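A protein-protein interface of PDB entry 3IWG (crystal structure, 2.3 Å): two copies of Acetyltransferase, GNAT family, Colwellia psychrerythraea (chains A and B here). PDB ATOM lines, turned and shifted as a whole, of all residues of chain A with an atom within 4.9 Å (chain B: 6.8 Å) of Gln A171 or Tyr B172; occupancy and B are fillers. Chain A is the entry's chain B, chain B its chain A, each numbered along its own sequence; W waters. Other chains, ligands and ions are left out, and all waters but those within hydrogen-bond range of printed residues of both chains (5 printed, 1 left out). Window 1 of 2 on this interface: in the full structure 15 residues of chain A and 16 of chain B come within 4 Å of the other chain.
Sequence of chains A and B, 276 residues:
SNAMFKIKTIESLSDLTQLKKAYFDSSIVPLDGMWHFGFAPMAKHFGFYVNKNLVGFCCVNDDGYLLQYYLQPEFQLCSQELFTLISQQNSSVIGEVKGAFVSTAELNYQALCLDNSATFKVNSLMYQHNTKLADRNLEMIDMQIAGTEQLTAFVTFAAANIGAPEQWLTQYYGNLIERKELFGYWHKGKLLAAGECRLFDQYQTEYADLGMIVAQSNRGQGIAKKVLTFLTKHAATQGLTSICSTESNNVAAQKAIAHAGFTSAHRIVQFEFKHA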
ATOM      1  N   GLN A 167     -26.508 -13.588 -34.996  1.00  0.00           N
ATOM      2  CA  GLN A 167     -26.981 -13.072 -33.742  1.00  0.00           C
ATOM      3  C   GLN A 167     -25.768 -12.800 -32.835  1.00  0.00           C
ATOM      4  O   GLN A 167     -25.646 -11.726 -32.226  1.00  0.00           O
ATOM      5  CB  GLN A 167     -27.911 -14.139 -33.126  1.00  0.00           C
ATOM      6  CG  GLN A 167     -29.158 -13.665 -32.528  1.00  0.00           C
ATOM      7  CD  GLN A 167     -29.986 -12.857 -33.474  1.00  0.00           C
ATOM      8  OE1 GLN A 167     -30.386 -11.746 -33.139  1.00  0.00           O
ATOM      9  NE2 GLN A 167     -30.227 -13.383 -34.674  1.00  0.00           N
ATOM     10  N   TRP A 168     -24.871 -13.776 -32.765  1.00  0.00           N
ATOM     11  CA  TRP A 168     -23.636 -13.640 -32.035  1.00  0.00           C
ATOM     12  C   TRP A 168     -22.765 -12.492 -32.592  1.00  0.00           C
ATOM     13  O   TRP A 168     -22.217 -11.683 -31.845  1.00  0.00           O
ATOM     14  CB  TRP A 168     -22.847 -14.948 -32.083  1.00  0.00           C
ATOM     15  CG  TRP A 168     -21.588 -14.920 -31.227  1.00  0.00           C
ATOM     16  CD1 TRP A 168     -21.507 -15.192 -29.902  1.00  0.00           C
ATOM     17  CD2 TRP A 168     -20.281 -14.561 -31.638  1.00  0.00           C
ATOM     18  NE1 TRP A 168     -20.234 -15.024 -29.457  1.00  0.00           N
ATOM     19  CE2 TRP A 168     -19.451 -14.652 -30.511  1.00  0.00           C
ATOM     20  CE3 TRP A 168     -19.724 -14.150 -32.852  1.00  0.00           C
ATOM     21  CZ2 TRP A 168     -18.100 -14.360 -30.559  1.00  0.00           C
ATOM     22  CZ3 TRP A 168     -18.411 -13.846 -32.901  1.00  0.00           C
ATOM     23  CH2 TRP A 168     -17.592 -13.979 -31.768  1.00  0.00           C
ATOM     24  N   LEU A 169     -22.638 -12.436 -33.912  1.00  0.00           N
ATOM     25  CA  LEU A 169     -21.772 -11.437 -34.554  1.00  0.00           C
ATOM     26  C   LEU A 169     -22.325 -10.045 -34.229  1.00  0.00           C
ATOM     27  O   LEU A 169     -21.570  -9.080 -34.069  1.00  0.00           O
ATOM     28  CB  LEU A 169     -21.752 -11.618 -36.067  1.00  0.00           C
ATOM     29  CG  LEU A 169     -20.604 -12.193 -36.882  1.00  0.00           C
ATOM     30  CD1 LEU A 169     -19.383 -12.635 -36.104  1.00  0.00           C
ATOM     31  CD2 LEU A 169     -21.175 -13.272 -37.779  1.00  0.00           C
ATOM     32  N   THR A 170     -23.641  -9.956 -34.140  1.00  0.00           N
ATOM     33  CA  THR A 170     -24.302  -8.666 -33.901  1.00  0.00           C
ATOM     34  C   THR A 170     -23.825  -8.120 -32.551  1.00  0.00           C
ATOM     35  O   THR A 170     -23.459  -6.932 -32.444  1.00  0.00           O
ATOM     36  CB  THR A 170     -25.817  -8.817 -33.999  1.00  0.00           C
ATOM     37  OG1 THR A 170     -26.145  -9.174 -35.358  1.00  0.00           O
ATOM     38  CG2 THR A 170     -26.605  -7.512 -33.612  1.00  0.00           C
ATOM     39  N   GLN A 171     -23.746  -8.999 -31.550  1.00  0.00           N
ATOM     40  CA  GLN A 171     -23.285  -8.600 -30.209  1.00  0.00           C
ATOM     41  C   GLN A 171     -21.788  -8.396 -30.197  1.00  0.00           C
ATOM     42  O   GLN A 171     -21.296  -7.440 -29.596  1.00  0.00           O
ATOM     43  CB  GLN A 171     -23.677  -9.640 -29.124  1.00  0.00           C
ATOM     44  CG  GLN A 171     -25.187  -9.706 -28.837  1.00  0.00           C
ATOM     45  CD  GLN A 171     -25.735  -8.400 -28.250  1.00  0.00           C
ATOM     46  OE1 GLN A 171     -25.129  -7.790 -27.370  1.00  0.00           O
ATOM     47  NE2 GLN A 171     -26.833  -7.948 -28.782  1.00  0.00           N
ATOM     48  N   TYR A 172     -21.068  -9.265 -30.876  1.00  0.00           N
ATOM     49  CA  TYR A 172     -19.603  -9.198 -30.810  1.00  0.00           C
ATOM     50  C   TYR A 172     -19.075  -7.898 -31.472  1.00  0.00           C
ATOM     51  O   TYR A 172     -18.246  -7.170 -30.904  1.00  0.00           O
ATOM     52  CB  TYR A 172     -18.974 -10.421 -31.496  1.00  0.00           C
ATOM     53  CG  TYR A 172     -17.473 -10.387 -31.597  1.00  0.00           C
ATOM     54  CD1 TYR A 172     -16.670 -10.680 -30.483  1.00  0.00           C
ATOM     55  CD2 TYR A 172     -16.816 -10.053 -32.822  1.00  0.00           C
ATOM     56  CE1 TYR A 172     -15.267 -10.678 -30.580  1.00  0.00           C
ATOM     57  CE2 TYR A 172     -15.438  -9.995 -32.900  1.00  0.00           C
ATOM     58  CZ  TYR A 172     -14.669 -10.331 -31.765  1.00  0.00           C
ATOM     59  OH  TYR A 172     -13.305 -10.322 -31.810  1.00  0.00           O
ATOM     60  N   TYR A 173     -19.540  -7.674 -32.696  1.00  0.00           N
ATOM     61  CA  TYR A 173     -19.211  -6.460 -33.447  1.00  0.00           C
ATOM     62  C   TYR A 173     -19.882  -5.217 -32.852  1.00  0.00           C
ATOM     63  O   TYR A 173     -19.283  -4.172 -32.839  1.00  0.00           O
ATOM     64  CB  TYR A 173     -19.655  -6.609 -34.899  1.00  0.00           C
ATOM     65  CG  TYR A 173     -18.795  -7.427 -35.800  1.00  0.00           C
ATOM     66  CD1 TYR A 173     -17.454  -7.643 -35.514  1.00  0.00           C
ATOM     67  CD2 TYR A 173     -19.274  -7.880 -37.028  1.00  0.00           C
ATOM     68  CE1 TYR A 173     -16.642  -8.280 -36.380  1.00  0.00           C
ATOM     69  CE2 TYR A 173     -18.426  -8.576 -37.920  1.00  0.00           C
ATOM     70  CZ  TYR A 173     -17.115  -8.763 -37.578  1.00  0.00           C
ATOM     71  OH  TYR A 173     -16.220  -9.444 -38.395  1.00  0.00           O
ATOM     72  N   GLY A 174     -21.083  -5.354 -32.290  1.00  0.00           N
ATOM     73  CA  GLY A 174     -21.725  -4.241 -31.546  1.00  0.00           C
ATOM     74  C   GLY A 174     -20.756  -3.732 -30.506  1.00  0.00           C
ATOM     75  O   GLY A 174     -20.444  -2.532 -30.414  1.00  0.00           O
ATOM     76  N   ASN A 175     -20.174  -4.663 -29.767  1.00  0.00           N
ATOM     77  CA  ASN A 175     -19.272  -4.280 -28.719  1.00  0.00           C
ATOM     78  C   ASN A 175     -17.992  -3.704 -29.243  1.00  0.00           C
ATOM     79  O   ASN A 175     -17.465  -2.746 -28.680  1.00  0.00           O
ATOM     80  CB  ASN A 175     -18.936  -5.466 -27.857  1.00  0.00           C
ATOM     81  CG  ASN A 175     -18.073  -5.078 -26.669  1.00  0.00           C
ATOM     82  OD1 ASN A 175     -18.481  -4.254 -25.829  1.00  0.00           O
ATOM     83  ND2 ASN A 175     -16.932  -5.678 -26.572  1.00  0.00           N
ATOM     84  N   MET B  34     -35.048  -3.024 -27.307  1.00  0.00           N
ATOM     85  CA  MET B  34     -34.642  -4.290 -27.947  1.00  0.00           C
ATOM     86  C   MET B  34     -35.282  -4.324 -29.316  1.00  0.00           C
ATOM     87  O   MET B  34     -34.614  -4.642 -30.281  1.00  0.00           O
ATOM     88  CB  MET B  34     -35.014  -5.547 -27.132  1.00  0.00           C
ATOM     89  CG  MET B  34     -33.848  -6.523 -26.888  1.00  0.00           C
ATOM     90  SD  MET B  34     -32.484  -6.882 -28.340  1.00  0.00           S
ATOM     91  CE  MET B  34     -30.900  -6.252 -27.369  1.00  0.00           C
ATOM     92  N   GLY B  38     -32.118  -3.069 -31.239  1.00  0.00           N
ATOM     93  CA  GLY B  38     -31.541  -4.409 -31.343  1.00  0.00           C
ATOM     94  C   GLY B  38     -32.026  -4.992 -32.644  1.00  0.00           C
ATOM     95  O   GLY B  38     -31.224  -5.114 -33.564  1.00  0.00           O
ATOM     96  N   LEU B 151     -18.773 -11.992 -14.920  1.00  0.00           N
ATOM     97  CA  LEU B 151     -19.557 -12.212 -16.141  1.00  0.00           C
ATOM     98  C   LEU B 151     -20.077 -13.618 -16.213  1.00  0.00           C
ATOM     99  O   LEU B 151     -21.235 -13.824 -16.593  1.00  0.00           O
ATOM    100  CB  LEU B 151     -18.736 -11.901 -17.392  1.00  0.00           C
ATOM    101  CG  LEU B 151     -19.292 -12.104 -18.806  1.00  0.00           C
ATOM    102  CD1 LEU B 151     -20.518 -11.234 -19.133  1.00  0.00           C
ATOM    103  CD2 LEU B 151     -18.133 -11.804 -19.824  1.00  0.00           C
ATOM    104  N   GLN B 167     -23.087 -18.304 -25.486  1.00  0.00           N
ATOM    105  CA  GLN B 167     -22.189 -17.520 -26.324  1.00  0.00           C
ATOM    106  C   GLN B 167     -22.756 -16.087 -26.480  1.00  0.00           C
ATOM    107  O   GLN B 167     -22.083 -15.084 -26.273  1.00  0.00           O
ATOM    108  CB  GLN B 167     -22.026 -18.166 -27.719  1.00  0.00           C
ATOM    109  CG  GLN B 167     -21.350 -19.543 -27.752  1.00  0.00           C
ATOM    110  CD  GLN B 167     -19.848 -19.448 -27.654  1.00  0.00           C
ATOM    111  OE1 GLN B 167     -19.304 -18.663 -26.849  1.00  0.00           O
ATOM    112  NE2 GLN B 167     -19.153 -20.225 -28.495  1.00  0.00           N
ATOM    113  N   TRP B 168     -24.015 -16.028 -26.839  1.00  0.00           N
ATOM    114  CA  TRP B 168     -24.743 -14.755 -26.960  1.00  0.00           C
ATOM    115  C   TRP B 168     -24.749 -13.907 -25.663  1.00  0.00           C
ATOM    116  O   TRP B 168     -24.352 -12.727 -25.657  1.00  0.00           O
ATOM    117  CB  TRP B 168     -26.155 -15.035 -27.397  1.00  0.00           C
ATOM    118  CG  TRP B 168     -26.835 -13.829 -27.824  1.00  0.00           C
ATOM    119  CD1 TRP B 168     -26.808 -13.285 -29.062  1.00  0.00           C
ATOM    120  CD2 TRP B 168     -27.640 -12.965 -27.017  1.00  0.00           C
ATOM    121  NE1 TRP B 168     -27.560 -12.157 -29.091  1.00  0.00           N
ATOM    122  CE2 TRP B 168     -28.065 -11.919 -27.843  1.00  0.00           C
ATOM    123  CE3 TRP B 168     -28.017 -12.964 -25.669  1.00  0.00           C
ATOM    124  CZ2 TRP B 168     -28.859 -10.896 -27.385  1.00  0.00           C
ATOM    125  CZ3 TRP B 168     -28.786 -11.965 -25.211  1.00  0.00           C
ATOM    126  CH2 TRP B 168     -29.233 -10.944 -26.063  1.00  0.00           C
ATOM    127  N   LEU B 169     -25.166 -14.537 -24.570  1.00  0.00           N
ATOM    128  CA  LEU B 169     -25.144 -13.904 -23.240  1.00  0.00           C
ATOM    129  C   LEU B 169     -23.770 -13.381 -22.875  1.00  0.00           C
ATOM    130  O   LEU B 169     -23.647 -12.299 -22.272  1.00  0.00           O
ATOM    131  CB  LEU B 169     -25.613 -14.878 -22.191  1.00  0.00           C
ATOM    132  CG  LEU B 169     -27.021 -14.918 -21.643  1.00  0.00           C
ATOM    133  CD1 LEU B 169     -27.981 -13.804 -22.051  1.00  0.00           C
ATOM    134  CD2 LEU B 169     -27.624 -16.304 -21.825  1.00  0.00           C
ATOM    135  N   THR B 170     -22.726 -14.107 -23.259  1.00  0.00           N
ATOM    136  CA  THR B 170     -21.379 -13.675 -22.936  1.00  0.00           C
ATOM    137  C   THR B 170     -21.085 -12.338 -23.596  1.00  0.00           C
ATOM    138  O   THR B 170     -20.492 -11.429 -22.985  1.00  0.00           O
ATOM    139  CB  THR B 170     -20.329 -14.744 -23.350  1.00  0.00           C
ATOM    140  OG1 THR B 170     -20.659 -15.994 -22.742  1.00  0.00           O
ATOM    141  CG2 THR B 170     -18.902 -14.343 -22.925  1.00  0.00           C
ATOM    142  N   GLN B 171     -21.542 -12.168 -24.831  1.00  0.00           N
ATOM    143  CA  GLN B 171     -21.316 -10.878 -25.503  1.00  0.00           C
ATOM    144  C   GLN B 171     -22.255  -9.814 -24.989  1.00  0.00           C
ATOM    145  O   GLN B 171     -21.852  -8.698 -24.724  1.00  0.00           O
ATOM    146  CB  GLN B 171     -21.451 -10.994 -27.031  1.00  0.00           C
ATOM    147  CG  GLN B 171     -20.344 -11.893 -27.710  1.00  0.00           C
ATOM    148  CD  GLN B 171     -18.911 -11.429 -27.448  1.00  0.00           C
ATOM    149  OE1 GLN B 171     -18.577 -10.246 -27.557  1.00  0.00           O
ATOM    150  NE2 GLN B 171     -18.054 -12.379 -27.142  1.00  0.00           N
ATOM    151  N   TYR B 172     -23.514 -10.147 -24.840  1.00  0.00           N
ATOM    152  CA  TYR B 172     -24.512  -9.137 -24.441  1.00  0.00           C
ATOM    153  C   TYR B 172     -24.202  -8.576 -23.054  1.00  0.00           C
ATOM    154  O   TYR B 172     -24.137  -7.363 -22.840  1.00  0.00           O
ATOM    155  CB  TYR B 172     -25.860  -9.782 -24.434  1.00  0.00           C
ATOM    156  CG  TYR B 172     -26.956  -8.911 -23.954  1.00  0.00           C
ATOM    157  CD1 TYR B 172     -27.616  -8.053 -24.824  1.00  0.00           C
ATOM    158  CD2 TYR B 172     -27.377  -8.973 -22.633  1.00  0.00           C
ATOM    159  CE1 TYR B 172     -28.637  -7.222 -24.349  1.00  0.00           C
ATOM    160  CE2 TYR B 172     -28.365  -8.153 -22.152  1.00  0.00           C
ATOM    161  CZ  TYR B 172     -28.992  -7.290 -23.005  1.00  0.00           C
ATOM    162  OH  TYR B 172     -29.995  -6.514 -22.542  1.00  0.00           O
ATOM    163  N   TYR B 173     -23.901  -9.490 -22.143  1.00  0.00           N
ATOM    164  CA  TYR B 173     -23.531  -9.121 -20.803  1.00  0.00           C
ATOM    165  C   TYR B 173     -22.149  -8.502 -20.724  1.00  0.00           C
ATOM    166  O   TYR B 173     -21.958  -7.580 -19.984  1.00  0.00           O
ATOM    167  CB  TYR B 173     -23.677 -10.310 -19.864  1.00  0.00           C
ATOM    168  CG  TYR B 173     -25.064 -10.622 -19.367  1.00  0.00           C
ATOM    169  CD1 TYR B 173     -26.056  -9.642 -19.244  1.00  0.00           C
ATOM    170  CD2 TYR B 173     -25.355 -11.900 -18.884  1.00  0.00           C
ATOM    171  CE1 TYR B 173     -27.325  -9.966 -18.714  1.00  0.00           C
ATOM    172  CE2 TYR B 173     -26.616 -12.226 -18.334  1.00  0.00           C
ATOM    173  CZ  TYR B 173     -27.577 -11.260 -18.247  1.00  0.00           C
ATOM    174  OH  TYR B 173     -28.770 -11.629 -17.692  1.00  0.00           O
ATOM    175  N   GLY B 174     -21.201  -8.938 -21.545  1.00  0.00           N
ATOM    176  CA  GLY B 174     -19.871  -8.293 -21.546  1.00  0.00           C
ATOM    177  C   GLY B 174     -19.980  -6.820 -21.888  1.00  0.00           C
ATOM    178  O   GLY B 174     -19.391  -5.925 -21.271  1.00  0.00           O
ATOM    179  N   ASN B 175     -20.772  -6.563 -22.898  1.00  0.00           N
ATOM    180  CA  ASN B 175     -21.031  -5.222 -23.295  1.00  0.00           C
ATOM    181  C   ASN B 175     -21.792  -4.441 -22.220  1.00  0.00           C
ATOM    182  O   ASN B 175     -21.465  -3.292 -21.958  1.00  0.00           O
ATOM    183  CB  ASN B 175     -21.795  -5.258 -24.595  1.00  0.00           C
ATOM    184  CG  ASN B 175     -21.978  -3.885 -25.188  1.00  0.00           C
ATOM    185  OD1 ASN B 175     -23.086  -3.449 -25.331  1.00  0.00           O
ATOM    186  ND2 ASN B 175     -20.876  -3.223 -25.557  1.00  0.00           N
ATOM    187  N   LEU B 176     -22.788  -5.030 -21.555  1.00  0.00           N
ATOM    188  CA  LEU B 176     -23.484  -4.260 -20.507  1.00  0.00           C
ATOM    189  C   LEU B 176     -22.540  -3.899 -19.345  1.00  0.00           C
ATOM    190  O   LEU B 176     -22.605  -2.807 -18.788  1.00  0.00           O
ATOM    191  CB  LEU B 176     -24.689  -5.011 -20.003  1.00  0.00           C
ATOM    192  CG  LEU B 176     -26.127  -4.770 -20.517  1.00  0.00           C
ATOM    193  CD1 LEU B 176     -26.300  -4.251 -21.932  1.00  0.00           C
ATOM    194  CD2 LEU B 176     -26.944  -6.021 -20.295  1.00  0.00           C
ATOM    195  N   ILE B 177     -21.643  -4.816 -19.006  1.00  0.00           N
ATOM    196  CA  ILE B 177     -20.705  -4.621 -17.930  1.00  0.00           C
ATOM    197  C   ILE B 177     -19.839  -3.400 -18.240  1.00  0.00           C
ATOM    198  O   ILE B 177     -19.668  -2.524 -17.376  1.00  0.00           O
ATOM    199  CB  ILE B 177     -19.850  -5.866 -17.757  1.00  0.00           C
ATOM    200  CG1 ILE B 177     -20.636  -6.953 -17.008  1.00  0.00           C
ATOM    201  CG2 ILE B 177     -18.519  -5.507 -17.047  1.00  0.00           C
ATOM    202  CD1 ILE B 177     -19.880  -8.177 -16.754  1.00  0.00           C
ATOM    203  N   LEU B 182     -25.318  -3.309 -15.806  1.00  0.00           N
ATOM    204  CA  LEU B 182     -25.776  -4.581 -15.248  1.00  0.00           C
ATOM    205  C   LEU B 182     -25.576  -4.604 -13.745  1.00  0.00           C
ATOM    206  O   LEU B 182     -24.536  -4.177 -13.268  1.00  0.00           O
ATOM    207  CB  LEU B 182     -25.048  -5.749 -15.914  1.00  0.00           C
ATOM    208  CG  LEU B 182     -25.365  -7.217 -15.500  1.00  0.00           C
ATOM    209  CD1 LEU B 182     -26.785  -7.635 -15.800  1.00  0.00           C
ATOM    210  CD2 LEU B 182     -24.360  -8.167 -16.199  1.00  0.00           C
ATOM    211  N   GLU B 196     -30.907  -4.814 -15.222  1.00  0.00           N
ATOM    212  CA  GLU B 196     -30.345  -3.989 -16.290  1.00  0.00           C
ATOM    213  C   GLU B 196     -30.970  -2.584 -16.282  1.00  0.00           C
ATOM    214  O   GLU B 196     -32.184  -2.449 -16.206  1.00  0.00           O
ATOM    215  CB  GLU B 196     -30.613  -4.630 -17.647  1.00  0.00           C
ATOM    216  CG  GLU B 196     -30.172  -6.074 -17.706  1.00  0.00           C
ATOM    217  CD  GLU B 196     -30.328  -6.752 -19.088  1.00  0.00           C
ATOM    218  OE1 GLU B 196     -30.691  -6.091 -20.093  1.00  0.00           O
ATOM    219  OE2 GLU B 196     -30.072  -7.972 -19.165  1.00  0.00           O
ATOM    220  N   ARG B 198     -30.461   0.308 -18.815  1.00  0.00           N
ATOM    221  CA  ARG B 198     -29.750   0.578 -20.051  1.00  0.00           C
ATOM    222  C   ARG B 198     -30.005   1.948 -20.568  1.00  0.00           C
ATOM    223  O   ARG B 198     -31.143   2.375 -20.652  1.00  0.00           O
ATOM    224  CB  ARG B 198     -30.238  -0.329 -21.139  1.00  0.00           C
ATOM    225  CG  ARG B 198     -30.136  -1.849 -20.875  1.00  0.00           C
ATOM    226  CD  ARG B 198     -30.978  -2.533 -21.990  1.00  0.00           C
ATOM    227  NE  ARG B 198     -31.508  -3.736 -21.447  1.00  0.00           N
ATOM    228  CZ  ARG B 198     -32.777  -4.065 -21.280  1.00  0.00           C
ATOM    229  NH1 ARG B 198     -33.015  -5.243 -20.706  1.00  0.00           N
ATOM    230  NH2 ARG B 198     -33.767  -3.328 -21.741  1.00  0.00           N
HETATM  231  O   HOH W   1     -28.208 -10.382 -31.322  1.00  0.00           O
HETATM  232  O   HOH W   2     -16.844  -8.122 -28.535  1.00  0.00           O
HETATM  233  O   HOH W   3     -19.261  -7.905 -25.898  1.00  0.00           O
HETATM  234  O   HOH W   4     -18.886 -15.238 -26.921  1.00  0.00           O
HETATM  235  O   HOH W   5     -22.630  -5.855 -27.716  1.00  0.00           O
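Of the 9 printed residues of chain A, 5 touch a printed residue of chain B.
Printed residues of chain A that touch a printed residue of chain B: Gln A167, Trp A168, Gln A171, Tyr A172 and Asn A175.
Hydrophobic or aromatic side chains of chain A within 4 Å of the printed part of chain B: Trp A168 and Tyr A172.
Hydrophobic or aromatic side chains of chain B that line the printed part of chain A: Trp B168 and Tyr B172.
Among the printed residues, 8 pairs touch across the chains.
Gln A171 touches just these residues of chain B: Trp B168, Gln B171 and Tyr B172.
Tyr B172 touches just one residue of chain A: Gln A171 (3.3 Å).
Printed residues of chain A within 4 Å of Trp B168: Gln A167 (3.7 Å) and Gln A171 (3.4 Å).
Printed residues of chain A within 4 Å of Gln B167: Trp A168 (3.7 Å).
Of the printed residues of chain A, Gln B171 touches Trp A168, Gln A171 and Tyr A172.
The nearest printed residue of chain A that does not touch Tyr B172 is Tyr A172 (6.6 Å).
The nearest printed residue of chain B that does not touch Tyr A172 is Tyr B172 (6.6 Å).
Gln A167 touches Trp B168, and with the chains exchanged Trp A168 touches Gln B167.
Trp A168 touches Gln B171, and with the chains exchanged Gln A171 touches Trp B168.
Gln A171 touches its own counterpart, Gln B171.
Asn B175 touches its own counterpart, Asn A175.
Of the 8 pairs that touch across the chains among the printed residues, 8 have their exchanged pair printed and touching as well.
Among the printed residues, merely in contact across the chains: Gln A171 with Tyr B172, Gln A171 with Gln B171, Gln A171 with Trp B168, Tyr A172 with Gln B171, Trp A168 with Gln B171, Trp A168 with Gln B167 and Gln A167 with Trp B168.
Water W5 lies within hydrogen-bond range of O of Gln A171 (2.8 Å), N of Asn A175 (3.4 Å) and OD1 of Asn B175 (3.4 Å).
Water W4 lies within hydrogen-bond range of the indole nitrogen (NE1) of Trp A168 (2.9 Å), the side-chain amide nitrogen (NE2) of Gln B171 (3.0 Å) and the backbone carbonyl oxygen (O) of Gln B167 (3.3 Å).
Water W2 lies within hydrogen-bond range of OE1 of Gln B171 (2.9 Å), O of Tyr A172 (2.9 Å) and ND2 of Asn A175 (3.1 Å).
Water W1 lies within hydrogen-bond range of the indole nitrogen of Trp B168 (2.9 Å) and the backbone carbonyl oxygen of Gln A167 (3.0 Å).
Water W3 bridges OE1 of Gln B171 and ND2 of Asn A175.
The side-chain amide oxygen (OD1) of Asn A175 lies within hydrogen-bond range of the side-chain amide nitrogen (ND2) of Asn B175, 2.6 Å away.
The side-chain hydroxyl of Tyr B172 is in hydrogen-bond range of the side-chain carboxylate of Glu B196 (2.6 Å).
OH of Tyr B172 sits at hydrogen-bond distance from NE of Arg B198 (3.3 Å).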
